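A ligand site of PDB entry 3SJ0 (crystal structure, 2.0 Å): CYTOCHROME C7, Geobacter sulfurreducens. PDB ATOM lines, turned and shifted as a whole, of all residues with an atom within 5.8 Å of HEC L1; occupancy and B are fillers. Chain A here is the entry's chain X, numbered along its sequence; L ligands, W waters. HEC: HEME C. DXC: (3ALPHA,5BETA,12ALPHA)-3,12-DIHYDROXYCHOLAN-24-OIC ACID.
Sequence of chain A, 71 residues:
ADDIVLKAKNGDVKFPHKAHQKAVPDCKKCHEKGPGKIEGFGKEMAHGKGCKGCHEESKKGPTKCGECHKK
A carbon (CAB) of HEC L1 is covalently linked to the side-chain sulfur (SG) of Cys 27 (2.0 Å).
A ring nitrogen (NE2) of His 31 is bound to an iron atom (FE) of HEC L1, at 2.0 Å.
SG of Cys 30 is covalently linked to CAC of HEC L1, at 2.0 Å.
NE2 of His 17 is bound to FE of HEC L1 (2.1 Å).
The backbone NH (N) of Ala 1 lies within hydrogen-bond range of an oxygen (O2A) of HEC L1 (2.6 Å).
A ring nitrogen (NE2) of His 20 binds an iron atom (FE) of HEC L2 (2.0 Å).
ND1 of His 17 sits close to OE1 of Gln 21 (3.3 Å).
The backbone NH (N) of His 17 lies within hydrogen-bond range of the side-chain carboxylate (OD1) of Asp 3 (3.1 Å).
O of Ile 4 lies within hydrogen-bond range of N of Phe 15 (3.0 Å).
A ring nitrogen (ND1) of His 20 sits at hydrogen-bond distance from the backbone carbonyl oxygen of Pro 16, at 2.7 Å.
An oxygen (O1D) of HEC L1 lies close to the backbone carbonyl oxygen (O) of Asp 2.
Merely in contact with HEC L1: Asp 3 (3.6 Å), Ile 4 (3.9 Å), Phe 15 (3.5 Å), His 20 (3.8 Å), Gln 21 (3.5 Å) and Val 24 (3.5 Å).
Hydrophobic or aromatic side chains that line HEC L1: Ala 1, Ile 4, Phe 15, His 17, His 20, Val 24 and His 31.
Of the 18 residues printed, 12 come within 4 Å of HEC L1.
The nearest printed residue that does not touch HEC L1 is Pro 25 (4.1 Å).
Water W2 lies within hydrogen-bond range of an oxygen (O1D) of HEC L1 and the side-chain carboxylate (OD1) of Asp 3.
Water W1 lies within hydrogen-bond range of O1A of HEC L1 (2.6 Å) and N of Ala 1 (3.4 Å).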
ATOM      1  N   ALA A   1     -12.803 -28.412  17.062  1.00  0.00           N
ATOM      2  CA  ALA A   1     -11.349 -28.571  16.750  1.00  0.00           C
ATOM      3  C   ALA A   1     -10.871 -29.925  17.229  1.00  0.00           C
ATOM      4  O   ALA A   1     -11.556 -30.634  17.980  1.00  0.00           O
ATOM      5  CB  ALA A   1     -10.542 -27.458  17.416  1.00  0.00           C
ATOM      6  N   ASP A   2      -9.687 -30.287  16.804  1.00  0.00           N
ATOM      7  CA  ASP A   2      -9.107 -31.566  17.137  1.00  0.00           C
ATOM      8  C   ASP A   2      -8.140 -31.455  18.285  1.00  0.00           C
ATOM      9  O   ASP A   2      -7.545 -30.399  18.489  1.00  0.00           O
ATOM     10  CB  ASP A   2      -8.393 -32.104  15.917  1.00  0.00           C
ATOM     11  CG  ASP A   2      -9.332 -32.371  14.805  1.00  0.00           C
ATOM     12  OD1 ASP A   2     -10.344 -33.119  15.057  1.00  0.00           O
ATOM     13  OD2 ASP A   2      -9.172 -31.854  13.671  1.00  0.00           O
ATOM     14  N   ASP A   3      -7.976 -32.536  19.021  1.00  0.00           N
ATOM     15  CA  ASP A   3      -6.910 -32.651  20.004  1.00  0.00           C
ATOM     16  C   ASP A   3      -5.550 -32.517  19.335  1.00  0.00           C
ATOM     17  O   ASP A   3      -5.407 -32.650  18.123  1.00  0.00           O
ATOM     18  CB  ASP A   3      -6.977 -33.962  20.776  1.00  0.00           C
ATOM     19  CG  ASP A   3      -8.155 -33.993  21.724  1.00  0.00           C
ATOM     20  OD1 ASP A   3      -8.705 -32.907  21.999  1.00  0.00           O
ATOM     21  OD2 ASP A   3      -8.576 -35.044  22.226  1.00  0.00           O
ATOM     22  N   ILE A   4      -4.546 -32.209  20.130  1.00  0.00           N
ATOM     23  CA  ILE A   4      -3.218 -32.121  19.593  1.00  0.00           C
ATOM     24  C   ILE A   4      -2.280 -33.079  20.300  1.00  0.00           C
ATOM     25  O   ILE A   4      -2.535 -33.508  21.422  1.00  0.00           O
ATOM     26  CB  ILE A   4      -2.720 -30.677  19.615  1.00  0.00           C
ATOM     27  CG1 ILE A   4      -2.738 -30.118  21.000  1.00  0.00           C
ATOM     28  CG2 ILE A   4      -3.580 -29.808  18.724  1.00  0.00           C
ATOM     29  CD1 ILE A   4      -2.317 -28.704  20.986  1.00  0.00           C
ATOM     30  N   PHE A  15      -2.867 -34.543  24.210  1.00  0.00           N
ATOM     31  CA  PHE A  15      -3.554 -33.585  25.051  1.00  0.00           C
ATOM     32  C   PHE A  15      -5.062 -33.659  24.747  1.00  0.00           C
ATOM     33  O   PHE A  15      -5.519 -33.130  23.709  1.00  0.00           O
ATOM     34  CB  PHE A  15      -3.046 -32.153  24.804  1.00  0.00           C
ATOM     35  CG  PHE A  15      -3.813 -31.141  25.604  1.00  0.00           C
ATOM     36  CD1 PHE A  15      -3.653 -31.071  26.983  1.00  0.00           C
ATOM     37  CD2 PHE A  15      -4.774 -30.341  24.989  1.00  0.00           C
ATOM     38  CE1 PHE A  15      -4.393 -30.182  27.737  1.00  0.00           C
ATOM     39  CE2 PHE A  15      -5.536 -29.463  25.741  1.00  0.00           C
ATOM     40  CZ  PHE A  15      -5.343 -29.360  27.102  1.00  0.00           C
ATOM     41  N   PRO A  16      -5.824 -34.350  25.596  1.00  0.00           N
ATOM     42  CA  PRO A  16      -7.281 -34.458  25.397  1.00  0.00           C
ATOM     43  C   PRO A  16      -8.072 -33.284  25.954  1.00  0.00           C
ATOM     44  O   PRO A  16      -8.212 -33.131  27.175  1.00  0.00           O
ATOM     45  CB  PRO A  16      -7.622 -35.759  26.137  1.00  0.00           C
ATOM     46  CG  PRO A  16      -6.615 -35.786  27.264  1.00  0.00           C
ATOM     47  CD  PRO A  16      -5.370 -35.116  26.766  1.00  0.00           C
ATOM     48  N   HIS A  17      -8.592 -32.433  25.055  1.00  0.00           N
ATOM     49  CA  HIS A  17      -9.249 -31.231  25.510  1.00  0.00           C
ATOM     50  C   HIS A  17     -10.517 -31.468  26.313  1.00  0.00           C
ATOM     51  O   HIS A  17     -10.725 -30.812  27.327  1.00  0.00           O
ATOM     52  CB  HIS A  17      -9.596 -30.256  24.365  1.00  0.00           C
ATOM     53  CG  HIS A  17     -10.039 -28.920  24.868  1.00  0.00           C
ATOM     54  ND1 HIS A  17     -11.355 -28.499  24.831  1.00  0.00           N
ATOM     55  CD2 HIS A  17      -9.351 -27.925  25.503  1.00  0.00           C
ATOM     56  CE1 HIS A  17     -11.441 -27.291  25.351  1.00  0.00           C
ATOM     57  NE2 HIS A  17     -10.244 -26.905  25.742  1.00  0.00           N
ATOM     58  N   HIS A  20     -10.133 -31.917  29.981  1.00  0.00           N
ATOM     59  CA  HIS A  20      -9.673 -30.732  30.672  1.00  0.00           C
ATOM     60  C   HIS A  20     -10.788 -29.695  30.834  1.00  0.00           C
ATOM     61  O   HIS A  20     -10.867 -29.031  31.855  1.00  0.00           O
ATOM     62  CB  HIS A  20      -8.476 -30.146  29.943  1.00  0.00           C
ATOM     63  CG  HIS A  20      -7.239 -30.958  30.123  1.00  0.00           C
ATOM     64  ND1 HIS A  20      -6.962 -32.041  29.332  1.00  0.00           N
ATOM     65  CD2 HIS A  20      -6.272 -30.892  31.056  1.00  0.00           C
ATOM     66  CE1 HIS A  20      -5.833 -32.597  29.744  1.00  0.00           C
ATOM     67  NE2 HIS A  20      -5.399 -31.923  30.792  1.00  0.00           N
ATOM     68  N   GLN A  21     -11.595 -29.541  29.815  1.00  0.00           N
ATOM     69  CA  GLN A  21     -12.720 -28.605  29.865  1.00  0.00           C
ATOM     70  C   GLN A  21     -13.666 -28.995  31.009  1.00  0.00           C
ATOM     71  O   GLN A  21     -14.145 -28.146  31.791  1.00  0.00           O
ATOM     72  CB  GLN A  21     -13.448 -28.647  28.528  1.00  0.00           C
ATOM     73  CG  GLN A  21     -14.495 -27.580  28.383  1.00  0.00           C
ATOM     74  CD  GLN A  21     -14.931 -27.397  26.932  1.00  0.00           C
ATOM     75  OE1 GLN A  21     -14.378 -28.180  26.046  1.00  0.00           O
ATOM     76  NE2 GLN A  21     -15.779 -26.564  26.642  1.00  0.00           N
ATOM     77  N   LYS A  22     -13.918 -30.288  31.115  1.00  0.00           N
ATOM     78  CA  LYS A  22     -14.741 -30.866  32.178  1.00  0.00           C
ATOM     79  C   LYS A  22     -14.108 -30.769  33.583  1.00  0.00           C
ATOM     80  O   LYS A  22     -14.790 -30.380  34.551  1.00  0.00           O
ATOM     81  CB  LYS A  22     -15.066 -32.327  31.857  1.00  0.00           C
ATOM     82  CG  LYS A  22     -15.979 -32.945  32.909  1.00  0.00           C
ATOM     83  CD  LYS A  22     -16.517 -34.284  32.462  1.00  0.00           C
ATOM     84  N   VAL A  24     -11.343 -28.944  34.576  1.00  0.00           N
ATOM     85  CA  VAL A  24     -10.708 -27.673  34.950  1.00  0.00           C
ATOM     86  C   VAL A  24     -11.640 -26.550  34.530  1.00  0.00           C
ATOM     87  O   VAL A  24     -11.382 -25.833  33.542  1.00  0.00           O
ATOM     88  CB  VAL A  24      -9.295 -27.523  34.301  1.00  0.00           C
ATOM     89  CG1 VAL A  24      -8.574 -26.299  34.838  1.00  0.00           C
ATOM     90  CG2 VAL A  24      -8.442 -28.770  34.554  1.00  0.00           C
ATOM     91  N   PRO A  25     -12.765 -26.410  35.239  1.00  0.00           N
ATOM     92  CA  PRO A  25     -13.750 -25.375  34.912  1.00  0.00           C
ATOM     93  C   PRO A  25     -13.242 -23.924  35.012  1.00  0.00           C
ATOM     94  O   PRO A  25     -13.797 -23.027  34.405  1.00  0.00           O
ATOM     95  CB  PRO A  25     -14.915 -25.669  35.895  1.00  0.00           C
ATOM     96  CG  PRO A  25     -14.291 -26.464  37.018  1.00  0.00           C
ATOM     97  CD  PRO A  25     -13.226 -27.287  36.339  1.00  0.00           C
ATOM     98  N   ASP A  26     -12.155 -23.715  35.728  1.00  0.00           N
ATOM     99  CA  ASP A  26     -11.442 -22.451  35.656  1.00  0.00           C
ATOM    100  C   ASP A  26     -10.645 -22.367  34.324  1.00  0.00           C
ATOM    101  O   ASP A  26      -9.442 -22.611  34.293  1.00  0.00           O
ATOM    102  CB  ASP A  26     -10.514 -22.316  36.854  1.00  0.00           C
ATOM    103  CG  ASP A  26     -10.050 -20.911  37.079  1.00  0.00           C
ATOM    104  OD1 ASP A  26     -10.099 -20.039  36.179  1.00  0.00           O
ATOM    105  OD2 ASP A  26      -9.599 -20.580  38.181  1.00  0.00           O
ATOM    106  N   CYS A  27     -11.314 -21.922  33.271  1.00  0.00           N
ATOM    107  CA  CYS A  27     -10.754 -21.861  31.910  1.00  0.00           C
ATOM    108  C   CYS A  27      -9.542 -20.962  31.834  1.00  0.00           C
ATOM    109  O   CYS A  27      -8.631 -21.226  31.046  1.00  0.00           O
ATOM    110  CB  CYS A  27     -11.804 -21.377  30.900  1.00  0.00           C
ATOM    111  SG  CYS A  27     -13.387 -22.231  31.002  1.00  0.00           S
ATOM    112  N   LYS A  29      -7.113 -20.813  33.697  1.00  0.00           N
ATOM    113  CA  LYS A  29      -5.851 -21.542  33.955  1.00  0.00           C
ATOM    114  C   LYS A  29      -5.041 -21.691  32.659  1.00  0.00           C
ATOM    115  O   LYS A  29      -3.812 -21.674  32.691  1.00  0.00           O
ATOM    116  CB  LYS A  29      -6.125 -22.904  34.586  1.00  0.00           C
ATOM    117  CG  LYS A  29      -6.427 -22.834  36.049  1.00  0.00           C
ATOM    118  CD  LYS A  29      -5.176 -22.370  36.788  1.00  0.00           C
ATOM    119  CE  LYS A  29      -5.193 -22.610  38.270  1.00  0.00           C
ATOM    120  NZ  LYS A  29      -3.941 -21.990  38.846  1.00  0.00           N
ATOM    121  N   CYS A  30      -5.724 -21.789  31.522  1.00  0.00           N
ATOM    122  CA  CYS A  30      -5.047 -21.946  30.241  1.00  0.00           C
ATOM    123  C   CYS A  30      -5.352 -20.899  29.190  1.00  0.00           C
ATOM    124  O   CYS A  30      -4.505 -20.653  28.318  1.00  0.00           O
ATOM    125  CB  CYS A  30      -5.426 -23.295  29.656  1.00  0.00           C
ATOM    126  SG  CYS A  30      -4.842 -24.650  30.688  1.00  0.00           S
ATOM    127  N   HIS A  31      -6.562 -20.335  29.246  1.00  0.00           N
ATOM    128  CA  HIS A  31      -7.018 -19.372  28.232  1.00  0.00           C
ATOM    129  C   HIS A  31      -6.942 -17.907  28.716  1.00  0.00           C
ATOM    130  O   HIS A  31      -6.889 -17.623  29.914  1.00  0.00           O
ATOM    131  CB  HIS A  31      -8.429 -19.739  27.734  1.00  0.00           C
ATOM    132  CG  HIS A  31      -8.513 -21.066  27.041  1.00  0.00           C
ATOM    133  ND1 HIS A  31      -7.770 -21.367  25.913  1.00  0.00           N
ATOM    134  CD2 HIS A  31      -9.236 -22.178  27.318  1.00  0.00           C
ATOM    135  CE1 HIS A  31      -8.032 -22.606  25.530  1.00  0.00           C
ATOM    136  NE2 HIS A  31      -8.922 -23.125  26.372  1.00  0.00           N
ATOM    137  N   GLY A  50       2.866 -26.232  33.311  1.00  0.00           N
ATOM    138  CA  GLY A  50       2.189 -26.461  32.046  1.00  0.00           C
ATOM    139  C   GLY A  50       1.425 -27.778  31.909  1.00  0.00           C
ATOM    140  O   GLY A  50       0.407 -27.839  31.200  1.00  0.00           O
HETATM  141 FE   HEC L   1      -9.599 -24.978  26.075  1.00  0.00          FE
HETATM  142  CHA HEC L   1      -9.194 -25.371  22.771  1.00  0.00           C
HETATM  143  CHB HEC L   1     -12.591 -23.451  25.536  1.00  0.00           C
HETATM  144  CHC HEC L   1     -10.351 -25.306  29.433  1.00  0.00           C
HETATM  145  CHD HEC L   1      -6.386 -25.708  26.693  1.00  0.00           C
HETATM  146  NA  HEC L   1     -10.656 -24.434  24.487  1.00  0.00           N
HETATM  147  C1A HEC L   1     -10.369 -24.836  23.196  1.00  0.00           C
HETATM  148  C2A HEC L   1     -11.517 -24.582  22.356  1.00  0.00           C
HETATM  149  C3A HEC L   1     -12.466 -24.038  23.114  1.00  0.00           C
HETATM  150  C4A HEC L   1     -11.936 -23.913  24.457  1.00  0.00           C
HETATM  151  CMA HEC L   1     -13.880 -23.591  22.641  1.00  0.00           C
HETATM  152  CAA HEC L   1     -11.672 -24.956  20.876  1.00  0.00           C
HETATM  153  CBA HEC L   1     -12.305 -26.364  20.990  1.00  0.00           C
HETATM  154  CGA HEC L   1     -12.940 -26.887  19.728  1.00  0.00           C
HETATM  155  O1A HEC L   1     -13.254 -26.085  18.791  1.00  0.00           O
HETATM  156  O2A HEC L   1     -13.114 -28.135  19.653  1.00  0.00           O
HETATM  157  NB  HEC L   1     -11.189 -24.532  27.274  1.00  0.00           N
HETATM  158  C1B HEC L   1     -12.319 -23.863  26.834  1.00  0.00           C
HETATM  159  C2B HEC L   1     -13.140 -23.584  27.975  1.00  0.00           C
HETATM  160  C3B HEC L   1     -12.541 -24.102  29.062  1.00  0.00           C
HETATM  161  C4B HEC L   1     -11.303 -24.702  28.632  1.00  0.00           C
HETATM  162  CMB HEC L   1     -14.493 -22.830  27.859  1.00  0.00           C
HETATM  163  CAB HEC L   1     -13.010 -24.123  30.527  1.00  0.00           C
HETATM  164  CBB HEC L   1     -14.140 -24.823  30.765  1.00  0.00           C
HETATM  165  NC  HEC L   1      -8.566 -25.405  27.731  1.00  0.00           N
HETATM  166  C1C HEC L   1      -9.046 -25.490  29.039  1.00  0.00           C
HETATM  167  C2C HEC L   1      -7.933 -25.823  29.902  1.00  0.00           C
HETATM  168  C3C HEC L   1      -6.845 -25.966  29.139  1.00  0.00           C
HETATM  169  C4C HEC L   1      -7.215 -25.683  27.781  1.00  0.00           C
HETATM  170  CMC HEC L   1      -8.029 -25.979  31.437  1.00  0.00           C
HETATM  171  CAC HEC L   1      -5.399 -26.290  29.615  1.00  0.00           C
HETATM  172  CBC HEC L   1      -5.181 -27.337  30.484  1.00  0.00           C
HETATM  173  ND  HEC L   1      -8.016 -25.444  24.888  1.00  0.00           N
HETATM  174  C1D HEC L   1      -6.769 -25.715  25.371  1.00  0.00           C
HETATM  175  C2D HEC L   1      -5.914 -26.027  24.257  1.00  0.00           C
HETATM  176  C3D HEC L   1      -6.769 -25.926  23.008  1.00  0.00           C
HETATM  177  C4D HEC L   1      -8.073 -25.549  23.522  1.00  0.00           C
HETATM  178  CMD HEC L   1      -4.454 -26.399  24.370  1.00  0.00           C
HETATM  179  CAD HEC L   1      -6.353 -26.228  21.547  1.00  0.00           C
HETATM  180  CBD HEC L   1      -6.053 -27.714  21.294  1.00  0.00           C
HETATM  181  CGD HEC L   1      -7.192 -28.683  21.577  1.00  0.00           C
HETATM  182  O1D HEC L   1      -8.328 -28.364  21.225  1.00  0.00           O
HETATM  183  O2D HEC L   1      -6.916 -29.791  22.111  1.00  0.00           O
HETATM  184 FE   HEC L   2      -4.079 -32.582  32.170  1.00  0.00          FE
HETATM  185  CHA HEC L   2      -6.152 -35.173  32.835  1.00  0.00           C
HETATM  186  CHB HEC L   2      -2.449 -34.496  29.780  1.00  0.00           C
HETATM  187  CHC HEC L   2      -2.190 -29.887  31.234  1.00  0.00           C
HETATM  188  CHD HEC L   2      -5.350 -30.811  34.771  1.00  0.00           C
HETATM  189  NA  HEC L   2      -4.254 -34.468  31.456  1.00  0.00           N
HETATM  190  C1A HEC L   2      -5.218 -35.365  31.851  1.00  0.00           C
HETATM  191  C2A HEC L   2      -5.101 -36.539  31.018  1.00  0.00           C
HETATM  192  C3A HEC L   2      -4.101 -36.358  30.184  1.00  0.00           C
HETATM  193  C4A HEC L   2      -3.532 -35.057  30.432  1.00  0.00           C
HETATM  194  CMA HEC L   2      -3.582 -37.379  29.133  1.00  0.00           C
HETATM  195  CAA HEC L   2      -6.001 -37.803  31.153  1.00  0.00           C
HETATM  196  CBA HEC L   2      -7.423 -37.489  30.743  1.00  0.00           C
HETATM  197  CGA HEC L   2      -8.262 -38.741  30.818  1.00  0.00           C
HETATM  198  O1A HEC L   2      -8.094 -39.534  31.782  1.00  0.00           O
HETATM  199  O2A HEC L   2      -9.095 -38.939  29.912  1.00  0.00           O
HETATM  200  NB  HEC L   2      -2.630 -32.261  30.771  1.00  0.00           N
HETATM  201  C1B HEC L   2      -2.047 -33.184  29.917  1.00  0.00           C
HETATM  202  C2B HEC L   2      -0.990 -32.533  29.157  1.00  0.00           C
HETATM  203  C3B HEC L   2      -0.947 -31.265  29.540  1.00  0.00           C
HETATM  204  C4B HEC L   2      -1.961 -31.064  30.559  1.00  0.00           C
HETATM  205  CMB HEC L   2      -0.101 -33.242  28.109  1.00  0.00           C
HETATM  206  CAB HEC L   2      -0.002 -30.167  29.024  1.00  0.00           C
HETATM  207  CBB HEC L   2       0.034 -29.916  27.684  1.00  0.00           C
HETATM  208  NC  HEC L   2      -3.792 -30.721  32.892  1.00  0.00           N
HETATM  209  C1C HEC L   2      -3.000 -29.748  32.350  1.00  0.00           C
HETATM  210  C2C HEC L   2      -3.169 -28.538  33.113  1.00  0.00           C
HETATM  211  C3C HEC L   2      -4.061 -28.789  34.079  1.00  0.00           C
HETATM  212  C4C HEC L   2      -4.455 -30.165  33.956  1.00  0.00           C
HETATM  213  CMC HEC L   2      -2.423 -27.226  32.806  1.00  0.00           C
HETATM  214  CAC HEC L   2      -4.619 -27.821  35.161  1.00  0.00           C
HETATM  215  CBC HEC L   2      -4.467 -26.494  35.020  1.00  0.00           C
HETATM  216  ND  HEC L   2      -5.524 -32.927  33.573  1.00  0.00           N
HETATM  217  C1D HEC L   2      -5.857 -32.062  34.607  1.00  0.00           C
HETATM  218  C2D HEC L   2      -6.867 -32.666  35.453  1.00  0.00           C
HETATM  219  C3D HEC L   2      -7.097 -34.034  34.851  1.00  0.00           C
HETATM  220  C4D HEC L   2      -6.234 -34.106  33.690  1.00  0.00           C
HETATM  221  CMD HEC L   2      -7.522 -32.116  36.730  1.00  0.00           C
HETATM  222  CAD HEC L   2      -8.060 -35.107  35.355  1.00  0.00           C
HETATM  223  CBD HEC L   2      -9.108 -35.353  34.292  1.00  0.00           C
HETATM  224  CGD HEC L   2      -9.818 -36.666  34.522  1.00  0.00           C
HETATM  225  O1D HEC L   2      -9.209 -37.654  35.015  1.00  0.00           O
HETATM  226  O2D HEC L   2     -11.022 -36.695  34.205  1.00  0.00           O
HETATM  227  C1  DXC L   3       2.890 -25.635  21.942  1.00  0.00           C
HETATM  228  C2  DXC L   3       2.096 -26.568  22.885  1.00  0.00           C
HETATM  229  C3  DXC L   3       0.587 -26.375  22.704  1.00  0.00           C
HETATM  230  C4  DXC L   3       0.152 -24.914  22.977  1.00  0.00           C
HETATM  231  C5  DXC L   3       1.011 -23.954  22.146  1.00  0.00           C
HETATM  232  C6  DXC L   3       2.509 -24.201  22.231  1.00  0.00           C
HETATM  233  C7  DXC L   3      -0.192 -27.393  23.564  1.00  0.00           C
HETATM  234  C8  DXC L   3      -0.028 -27.052  25.058  1.00  0.00           C
HETATM  235  C9  DXC L   3      -0.504 -25.590  25.336  1.00  0.00           C
HETATM  236  C10 DXC L   3       0.276 -24.586  24.472  1.00  0.00           C
HETATM  237  C11 DXC L   3      -0.319 -25.200  26.801  1.00  0.00           C
HETATM  238  C12 DXC L   3      -0.842 -23.807  27.159  1.00  0.00           C
HETATM  239  C13 DXC L   3      -0.063 -22.783  26.349  1.00  0.00           C
HETATM  240  C14 DXC L   3      -0.093 -23.102  24.820  1.00  0.00           C
HETATM  241  C15 DXC L   3      -1.021 -26.111  27.831  1.00  0.00           C
HETATM  242  C16 DXC L   3      -1.014 -25.259  29.105  1.00  0.00           C
HETATM  243  C17 DXC L   3      -0.527 -23.845  28.689  1.00  0.00           C
HETATM  244  C18 DXC L   3      -1.290 -24.741  22.458  1.00  0.00           C
HETATM  245  C19 DXC L   3      -1.232 -22.783  29.572  1.00  0.00           C
HETATM  246  O1  DXC L   3       1.294 -22.812  26.753  1.00  0.00           O
HETATM  247  O2  DXC L   3       4.305 -25.823  22.139  1.00  0.00           O
HETATM  248  C20 DXC L   3      -2.333 -23.629  26.841  1.00  0.00           C
HETATM  249  C21 DXC L   3      -1.053 -23.093  31.051  1.00  0.00           C
HETATM  250  C22 DXC L   3       0.410 -23.187  31.447  1.00  0.00           C
HETATM  251  C23 DXC L   3       0.954 -21.861  31.962  1.00  0.00           C
HETATM  252  O3  DXC L   3       0.484 -21.354  32.982  1.00  0.00           O
HETATM  253  O4  DXC L   3       1.884 -21.311  31.350  1.00  0.00           O
HETATM  254  C24 DXC L   3      -0.827 -21.324  29.263  1.00  0.00           C
HETATM  255  O   HOH W   1     -15.611 -26.540  17.678  1.00  0.00           O
HETATM  256  O   HOH W   2      -9.920 -30.340  21.087  1.00  0.00           O
